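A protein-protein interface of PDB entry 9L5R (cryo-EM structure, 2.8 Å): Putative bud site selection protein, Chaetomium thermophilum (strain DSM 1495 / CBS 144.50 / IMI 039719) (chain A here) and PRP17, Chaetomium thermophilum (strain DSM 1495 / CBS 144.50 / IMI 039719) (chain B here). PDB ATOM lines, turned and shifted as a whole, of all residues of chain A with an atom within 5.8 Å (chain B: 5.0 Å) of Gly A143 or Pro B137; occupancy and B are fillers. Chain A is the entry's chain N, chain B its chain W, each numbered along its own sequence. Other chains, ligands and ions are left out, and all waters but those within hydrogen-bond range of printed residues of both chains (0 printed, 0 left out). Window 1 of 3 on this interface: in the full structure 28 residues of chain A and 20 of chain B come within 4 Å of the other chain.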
ATOM      1  N   HIS A  56      13.275  -0.362   3.583  1.00  0.00           N
ATOM      2  CA  HIS A  56      13.276  -0.548   2.137  1.00  0.00           C
ATOM      3  C   HIS A  56      14.608  -1.094   1.652  1.00  0.00           C
ATOM      4  O   HIS A  56      14.636  -1.993   0.811  1.00  0.00           O
ATOM      5  CB  HIS A  56      12.950   0.778   1.446  1.00  0.00           C
ATOM      6  CG  HIS A  56      12.925   0.721  -0.054  1.00  0.00           C
ATOM      7  ND1 HIS A  56      11.797   1.014  -0.783  1.00  0.00           N
ATOM      8  CD2 HIS A  56      13.895   0.463  -0.961  1.00  0.00           C
ATOM      9  CE1 HIS A  56      12.066   0.908  -2.070  1.00  0.00           C
ATOM     10  NE2 HIS A  56      13.332   0.569  -2.205  1.00  0.00           N
ATOM     11  N   LYS A 101       9.281  -0.057  -7.714  1.00  0.00           N
ATOM     12  CA  LYS A 101      10.224   0.752  -6.915  1.00  0.00           C
ATOM     13  C   LYS A 101       9.513   1.384  -5.728  1.00  0.00           C
ATOM     14  O   LYS A 101      10.020   2.373  -5.247  1.00  0.00           O
ATOM     15  CB  LYS A 101      10.807   1.841  -7.808  1.00  0.00           C
ATOM     16  CG  LYS A 101      11.786   1.383  -8.875  1.00  0.00           C
ATOM     17  CD  LYS A 101      11.889   2.350 -10.027  1.00  0.00           C
ATOM     18  CE  LYS A 101      12.614   1.758 -11.214  1.00  0.00           C
ATOM     19  NZ  LYS A 101      13.081   2.805 -12.149  1.00  0.00           N
ATOM     20  N   LEU A 102       8.397   0.829  -5.265  1.00  0.00           N
ATOM     21  CA  LEU A 102       7.585   1.436  -4.180  1.00  0.00           C
ATOM     22  C   LEU A 102       8.434   1.658  -2.942  1.00  0.00           C
ATOM     23  O   LEU A 102       9.175   0.769  -2.594  1.00  0.00           O
ATOM     24  CB  LEU A 102       6.399   0.524  -3.883  1.00  0.00           C
ATOM     25  CG  LEU A 102       5.496   0.937  -2.734  1.00  0.00           C
ATOM     26  CD1 LEU A 102       4.833   2.262  -3.032  1.00  0.00           C
ATOM     27  CD2 LEU A 102       4.456  -0.132  -2.485  1.00  0.00           C
ATOM     28  N   CYS A 103       8.284   2.799  -2.294  1.00  0.00           N
ATOM     29  CA  CYS A 103       9.039   3.133  -1.080  1.00  0.00           C
ATOM     30  C   CYS A 103       8.436   2.409   0.107  1.00  0.00           C
ATOM     31  O   CYS A 103       9.206   1.872   0.900  1.00  0.00           O
ATOM     32  CB  CYS A 103       8.937   4.622  -0.811  1.00  0.00           C
ATOM     33  SG  CYS A 103       7.282   5.320  -0.994  1.00  0.00           S
ATOM     34  N   CYS A 121       4.205  10.908  -4.219  1.00  0.00           N
ATOM     35  CA  CYS A 121       5.516  10.341  -4.600  1.00  0.00           C
ATOM     36  C   CYS A 121       5.335   9.232  -5.623  1.00  0.00           C
ATOM     37  O   CYS A 121       6.308   8.883  -6.280  1.00  0.00           O
ATOM     38  CB  CYS A 121       6.255   9.846  -3.375  1.00  0.00           C
ATOM     39  SG  CYS A 121       5.677   8.289  -2.682  1.00  0.00           S
ATOM     40  N   VAL A 123       3.432   9.606  -8.227  1.00  0.00           N
ATOM     41  CA  VAL A 123       3.044  10.264  -9.503  1.00  0.00           C
ATOM     42  C   VAL A 123       4.276  10.400 -10.378  1.00  0.00           C
ATOM     43  O   VAL A 123       5.294  10.863  -9.870  1.00  0.00           O
ATOM     44  CB  VAL A 123       2.402  11.632  -9.241  1.00  0.00           C
ATOM     45  CG1 VAL A 123       2.052  12.375 -10.517  1.00  0.00           C
ATOM     46  CG2 VAL A 123       1.184  11.485  -8.362  1.00  0.00           C
ATOM     47  N   ARG A 125       7.064  11.917 -12.237  1.00  0.00           N
ATOM     48  CA  ARG A 125       7.585  13.279 -12.209  1.00  0.00           C
ATOM     49  C   ARG A 125       7.455  13.999 -13.538  1.00  0.00           C
ATOM     50  O   ARG A 125       7.703  15.206 -13.592  1.00  0.00           O
ATOM     51  CB  ARG A 125       9.039  13.280 -11.750  1.00  0.00           C
ATOM     52  CG  ARG A 125       9.149  12.788 -10.332  1.00  0.00           C
ATOM     53  CD  ARG A 125       8.528  13.818  -9.421  1.00  0.00           C
ATOM     54  NE  ARG A 125       8.655  13.510  -8.004  1.00  0.00           N
ATOM     55  CZ  ARG A 125       7.759  12.823  -7.309  1.00  0.00           C
ATOM     56  NH1 ARG A 125       6.707  12.273  -7.893  1.00  0.00           N
ATOM     57  NH2 ARG A 125       7.922  12.683  -6.000  1.00  0.00           N
ATOM     58  N   ILE A 134       9.436  17.199  -4.234  1.00  0.00           N
ATOM     59  CA  ILE A 134       8.564  16.428  -3.362  1.00  0.00           C
ATOM     60  C   ILE A 134       9.411  15.603  -2.411  1.00  0.00           C
ATOM     61  O   ILE A 134      10.370  14.945  -2.827  1.00  0.00           O
ATOM     62  CB  ILE A 134       7.626  15.530  -4.182  1.00  0.00           C
ATOM     63  CG1 ILE A 134       6.755  16.371  -5.115  1.00  0.00           C
ATOM     64  CG2 ILE A 134       6.836  14.606  -3.291  1.00  0.00           C
ATOM     65  CD1 ILE A 134       5.866  17.344  -4.386  1.00  0.00           C
ATOM     66  N   GLY A 140       9.387  10.351   3.079  1.00  0.00           N
ATOM     67  CA  GLY A 140      10.397  11.270   2.541  1.00  0.00           C
ATOM     68  C   GLY A 140      10.846  10.861   1.172  1.00  0.00           C
ATOM     69  O   GLY A 140      11.928  11.267   0.791  1.00  0.00           O
ATOM     70  N   CYS A 141      10.023  10.121   0.450  1.00  0.00           N
ATOM     71  CA  CYS A 141      10.407   9.598  -0.878  1.00  0.00           C
ATOM     72  C   CYS A 141      10.329  10.727  -1.884  1.00  0.00           C
ATOM     73  O   CYS A 141       9.381  11.507  -1.815  1.00  0.00           O
ATOM     74  CB  CYS A 141       9.483   8.455  -1.246  1.00  0.00           C
ATOM     75  SG  CYS A 141       9.285   8.100  -2.998  1.00  0.00           S
ATOM     76  N   ARG A 142      11.294  10.794  -2.784  1.00  0.00           N
ATOM     77  CA  ARG A 142      11.349  11.925  -3.723  1.00  0.00           C
ATOM     78  C   ARG A 142      10.775  11.510  -5.073  1.00  0.00           C
ATOM     79  O   ARG A 142      10.757  12.356  -5.958  1.00  0.00           O
ATOM     80  CB  ARG A 142      12.804  12.367  -3.808  1.00  0.00           C
ATOM     81  CG  ARG A 142      13.471  12.540  -2.456  1.00  0.00           C
ATOM     82  CD  ARG A 142      14.844  13.116  -2.679  1.00  0.00           C
ATOM     83  NE  ARG A 142      15.452  13.623  -1.467  1.00  0.00           N
ATOM     84  CZ  ARG A 142      15.483  14.902  -1.134  1.00  0.00           C
ATOM     85  NH1 ARG A 142      14.928  15.807  -1.921  1.00  0.00           N
ATOM     86  NH2 ARG A 142      16.060  15.275  -0.009  1.00  0.00           N
ATOM     87  N   GLY A 143      10.318  10.270  -5.217  1.00  0.00           N
ATOM     88  CA  GLY A 143       9.808   9.757  -6.500  1.00  0.00           C
ATOM     89  C   GLY A 143       9.932   8.259  -6.551  1.00  0.00           C
ATOM     90  O   GLY A 143      11.052   7.769  -6.553  1.00  0.00           O
ATOM     91  N   CYS A 144       8.818   7.554  -6.595  1.00  0.00           N
ATOM     92  CA  CYS A 144       8.815   6.080  -6.547  1.00  0.00           C
ATOM     93  C   CYS A 144       8.351   5.488  -7.849  1.00  0.00           C
ATOM     94  O   CYS A 144       8.569   4.302  -8.043  1.00  0.00           O
ATOM     95  CB  CYS A 144       7.597   5.663  -5.769  1.00  0.00           C
ATOM     96  SG  CYS A 144       7.982   4.999  -4.157  1.00  0.00           S
ATOM     97  N   ALA A 145       7.624   6.262  -8.638  1.00  0.00           N
ATOM     98  CA  ALA A 145       7.016   5.713  -9.863  1.00  0.00           C
ATOM     99  C   ALA A 145       8.046   4.894 -10.620  1.00  0.00           C
ATOM    100  O   ALA A 145       9.219   5.265 -10.642  1.00  0.00           O
ATOM    101  CB  ALA A 145       6.466   6.828 -10.693  1.00  0.00           C
ATOM    102  N   ASP A 148      10.042   6.822 -13.087  1.00  0.00           N
ATOM    103  CA  ASP A 148      11.038   7.622 -12.382  1.00  0.00           C
ATOM    104  C   ASP A 148      12.245   6.797 -11.952  1.00  0.00           C
ATOM    105  O   ASP A 148      13.131   7.296 -11.264  1.00  0.00           O
ATOM    106  CB  ASP A 148      10.424   8.280 -11.150  1.00  0.00           C
ATOM    107  CG  ASP A 148       9.246   9.162 -11.482  1.00  0.00           C
ATOM    108  OD1 ASP A 148       9.029   9.454 -12.674  1.00  0.00           O
ATOM    109  OD2 ASP A 148       8.531   9.558 -10.542  1.00  0.00           O
ATOM    110  OXT ASP A 148      12.374   5.616 -12.262  1.00  0.00           O
ATOM    111  N   ARG B 119      17.857  12.746 -12.482  1.00  0.00           N
ATOM    112  CA  ARG B 119      17.919  12.235 -11.118  1.00  0.00           C
ATOM    113  C   ARG B 119      19.284  11.608 -10.845  1.00  0.00           C
ATOM    114  O   ARG B 119      19.988  11.171 -11.757  1.00  0.00           O
ATOM    115  CB  ARG B 119      16.815  11.208 -10.878  1.00  0.00           C
ATOM    116  CG  ARG B 119      16.356  11.113  -9.434  1.00  0.00           C
ATOM    117  CD  ARG B 119      15.354  10.005  -9.259  1.00  0.00           C
ATOM    118  NE  ARG B 119      14.850   9.941  -7.895  1.00  0.00           N
ATOM    119  CZ  ARG B 119      13.634   9.534  -7.568  1.00  0.00           C
ATOM    120  NH1 ARG B 119      12.780   9.108  -8.478  1.00  0.00           N
ATOM    121  NH2 ARG B 119      13.265   9.561  -6.293  1.00  0.00           N
ATOM    122  N   TYR B 134      22.412   1.326  -1.992  1.00  0.00           N
ATOM    123  CA  TYR B 134      21.099   1.643  -2.529  1.00  0.00           C
ATOM    124  C   TYR B 134      20.517   2.854  -1.822  1.00  0.00           C
ATOM    125  O   TYR B 134      20.531   2.932  -0.594  1.00  0.00           O
ATOM    126  CB  TYR B 134      20.172   0.447  -2.366  1.00  0.00           C
ATOM    127  CG  TYR B 134      18.870   0.550  -3.109  1.00  0.00           C
ATOM    128  CD1 TYR B 134      18.845   0.720  -4.474  1.00  0.00           C
ATOM    129  CD2 TYR B 134      17.666   0.469  -2.441  1.00  0.00           C
ATOM    130  CE1 TYR B 134      17.657   0.816  -5.152  1.00  0.00           C
ATOM    131  CE2 TYR B 134      16.480   0.572  -3.109  1.00  0.00           C
ATOM    132  CZ  TYR B 134      16.477   0.736  -4.461  1.00  0.00           C
ATOM    133  OH  TYR B 134      15.283   0.836  -5.131  1.00  0.00           O
ATOM    134  N   ILE B 135      20.023   3.812  -2.598  1.00  0.00           N
ATOM    135  CA  ILE B 135      19.187   4.868  -2.051  1.00  0.00           C
ATOM    136  C   ILE B 135      17.813   4.919  -2.697  1.00  0.00           C
ATOM    137  O   ILE B 135      16.873   5.420  -2.062  1.00  0.00           O
ATOM    138  CB  ILE B 135      19.874   6.247  -2.140  1.00  0.00           C
ATOM    139  CG1 ILE B 135      20.112   6.658  -3.580  1.00  0.00           C
ATOM    140  CG2 ILE B 135      21.195   6.231  -1.415  1.00  0.00           C
ATOM    141  CD1 ILE B 135      20.616   8.056  -3.705  1.00  0.00           C
ATOM    142  N   GLY B 136      17.699   4.331  -3.876  1.00  0.00           N
ATOM    143  CA  GLY B 136      16.405   4.176  -4.546  1.00  0.00           C
ATOM    144  C   GLY B 136      15.529   5.377  -4.603  1.00  0.00           C
ATOM    145  O   GLY B 136      15.982   6.424  -5.012  1.00  0.00           O
ATOM    146  N   PRO B 137      14.255   5.239  -4.231  1.00  0.00           N
ATOM    147  CA  PRO B 137      13.320   6.330  -4.375  1.00  0.00           C
ATOM    148  C   PRO B 137      13.688   7.590  -3.589  1.00  0.00           C
ATOM    149  O   PRO B 137      13.017   8.568  -3.753  1.00  0.00           O
ATOM    150  CB  PRO B 137      12.067   5.706  -3.776  1.00  0.00           C
ATOM    151  CG  PRO B 137      12.232   4.240  -3.973  1.00  0.00           C
ATOM    152  CD  PRO B 137      13.690   4.021  -3.677  1.00  0.00           C
ATOM    153  N   TRP B 138      14.698   7.519  -2.731  1.00  0.00           N
ATOM    154  CA  TRP B 138      15.115   8.680  -1.917  1.00  0.00           C
ATOM    155  C   TRP B 138      16.254   9.395  -2.627  1.00  0.00           C
ATOM    156  O   TRP B 138      16.870  10.259  -2.013  1.00  0.00           O
ATOM    157  CB  TRP B 138      15.500   8.217  -0.524  1.00  0.00           C
ATOM    158  CG  TRP B 138      14.316   7.789   0.276  1.00  0.00           C
ATOM    159  CD1 TRP B 138      13.529   8.579   1.053  1.00  0.00           C
ATOM    160  CD2 TRP B 138      13.767   6.468   0.355  1.00  0.00           C
ATOM    161  NE1 TRP B 138      12.529   7.838   1.612  1.00  0.00           N
ATOM    162  CE2 TRP B 138      12.649   6.540   1.205  1.00  0.00           C
ATOM    163  CE3 TRP B 138      14.114   5.236  -0.199  1.00  0.00           C
ATOM    164  CZ2 TRP B 138      11.875   5.428   1.512  1.00  0.00           C
ATOM    165  CZ3 TRP B 138      13.348   4.138   0.101  1.00  0.00           C
ATOM    166  CH2 TRP B 138      12.245   4.235   0.945  1.00  0.00           C
ATOM    167  N   ALA B 139      16.502   9.052  -3.883  1.00  0.00           N
ATOM    168  CA  ALA B 139      17.511   9.740  -4.668  1.00  0.00           C
ATOM    169  C   ALA B 139      17.073  11.163  -4.971  1.00  0.00           C
ATOM    170  O   ALA B 139      15.925  11.409  -5.344  1.00  0.00           O
ATOM    171  CB  ALA B 139      17.764   8.985  -5.966  1.00  0.00           C
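Printed residues of chain A that touch a printed residue of chain B: His A56, Lys A101, Cys A103, Gly A140, Cys A141, Arg A142, Gly A143 and Asp A148. Of the 7 printed residues of chain B, 5 touch a printed residue of chain A. Hydrophobic or aromatic side chains of chain B that line the printed part of chain A: Tyr B134, Pro B137 and Trp B138. Among the printed residues, 15 pairs touch across the chains.
O of Gly A143 sits at hydrogen-bond distance from NH2 of Arg B119, 2.9 Å away. The backbone NH (N) of Arg A142 is in hydrogen-bond range of the backbone carbonyl oxygen (O) of Pro B137 (3.0 Å). The chain-end carboxylate of Asp A148 is in salt-bridge range of the guanidinium group of Arg B119, at 3.3 Å.
Tyr B134 touches His A56. His A56 touches Trp B138 (CG to CZ3, 3.4 Å). O of Lys A101 touches CG of Pro B137, at 3.2 Å. Cys A103 touches Trp B138 (CB to CH2, 3.8 Å). Trp B138 touches Gly A140 (CD1 to O, 3.1 Å). Cys A141 touches Pro B137. Trp B138 touches Cys A141 (NE1 to N, 3.6 Å). Arg A142 touches Arg B119 (C to NH2, 3.4 Å). Arg A142 touches Trp B138 (CD to O, 3.6 Å). Gly A143 touches Pro B137.
Of chain B, only Arg B119 and Pro B137 come within 4 Å of Gly A143. Printed residues of chain B within 4 Å of Asp A148: Arg B119. Pro B137 touches just these residues of chain A: His A56, Lys A101, Cys A141, Arg A142 and Gly A143. Of the printed residues of chain A, Trp B138 touches His A56 (3.4 Å), Cys A103 (3.8 Å), Gly A140 (3.1 Å), Cys A141 (3.6 Å) and Arg A142 (3.6 Å). The nearest printed residue of chain B that does not touch Gly A143 is Trp B138 (5.3 Å).
The chain-end carboxylate (OXT) of Asp A148 is in salt-bridge range of the side-chain amino group (NZ) of Lys A101. NE of Arg B119 lies within hydrogen-bond range of O of Ala B139. ND1 of His A56 lies within hydrogen-bond range of O of Cys A103, 3.2 Å away. N of Gly A143 lies close to SG of Cys A141 (3.3 Å). The backbone carbonyl oxygen (O) of Arg A142 sits at hydrogen-bond distance from the guanidinium group (NH2) of Arg A125 (2.9 Å). The backbone NH (N) of Arg A125 lies within hydrogen-bond range of the side-chain carboxylate (OD1) of Asp A148 (3.2 Å).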
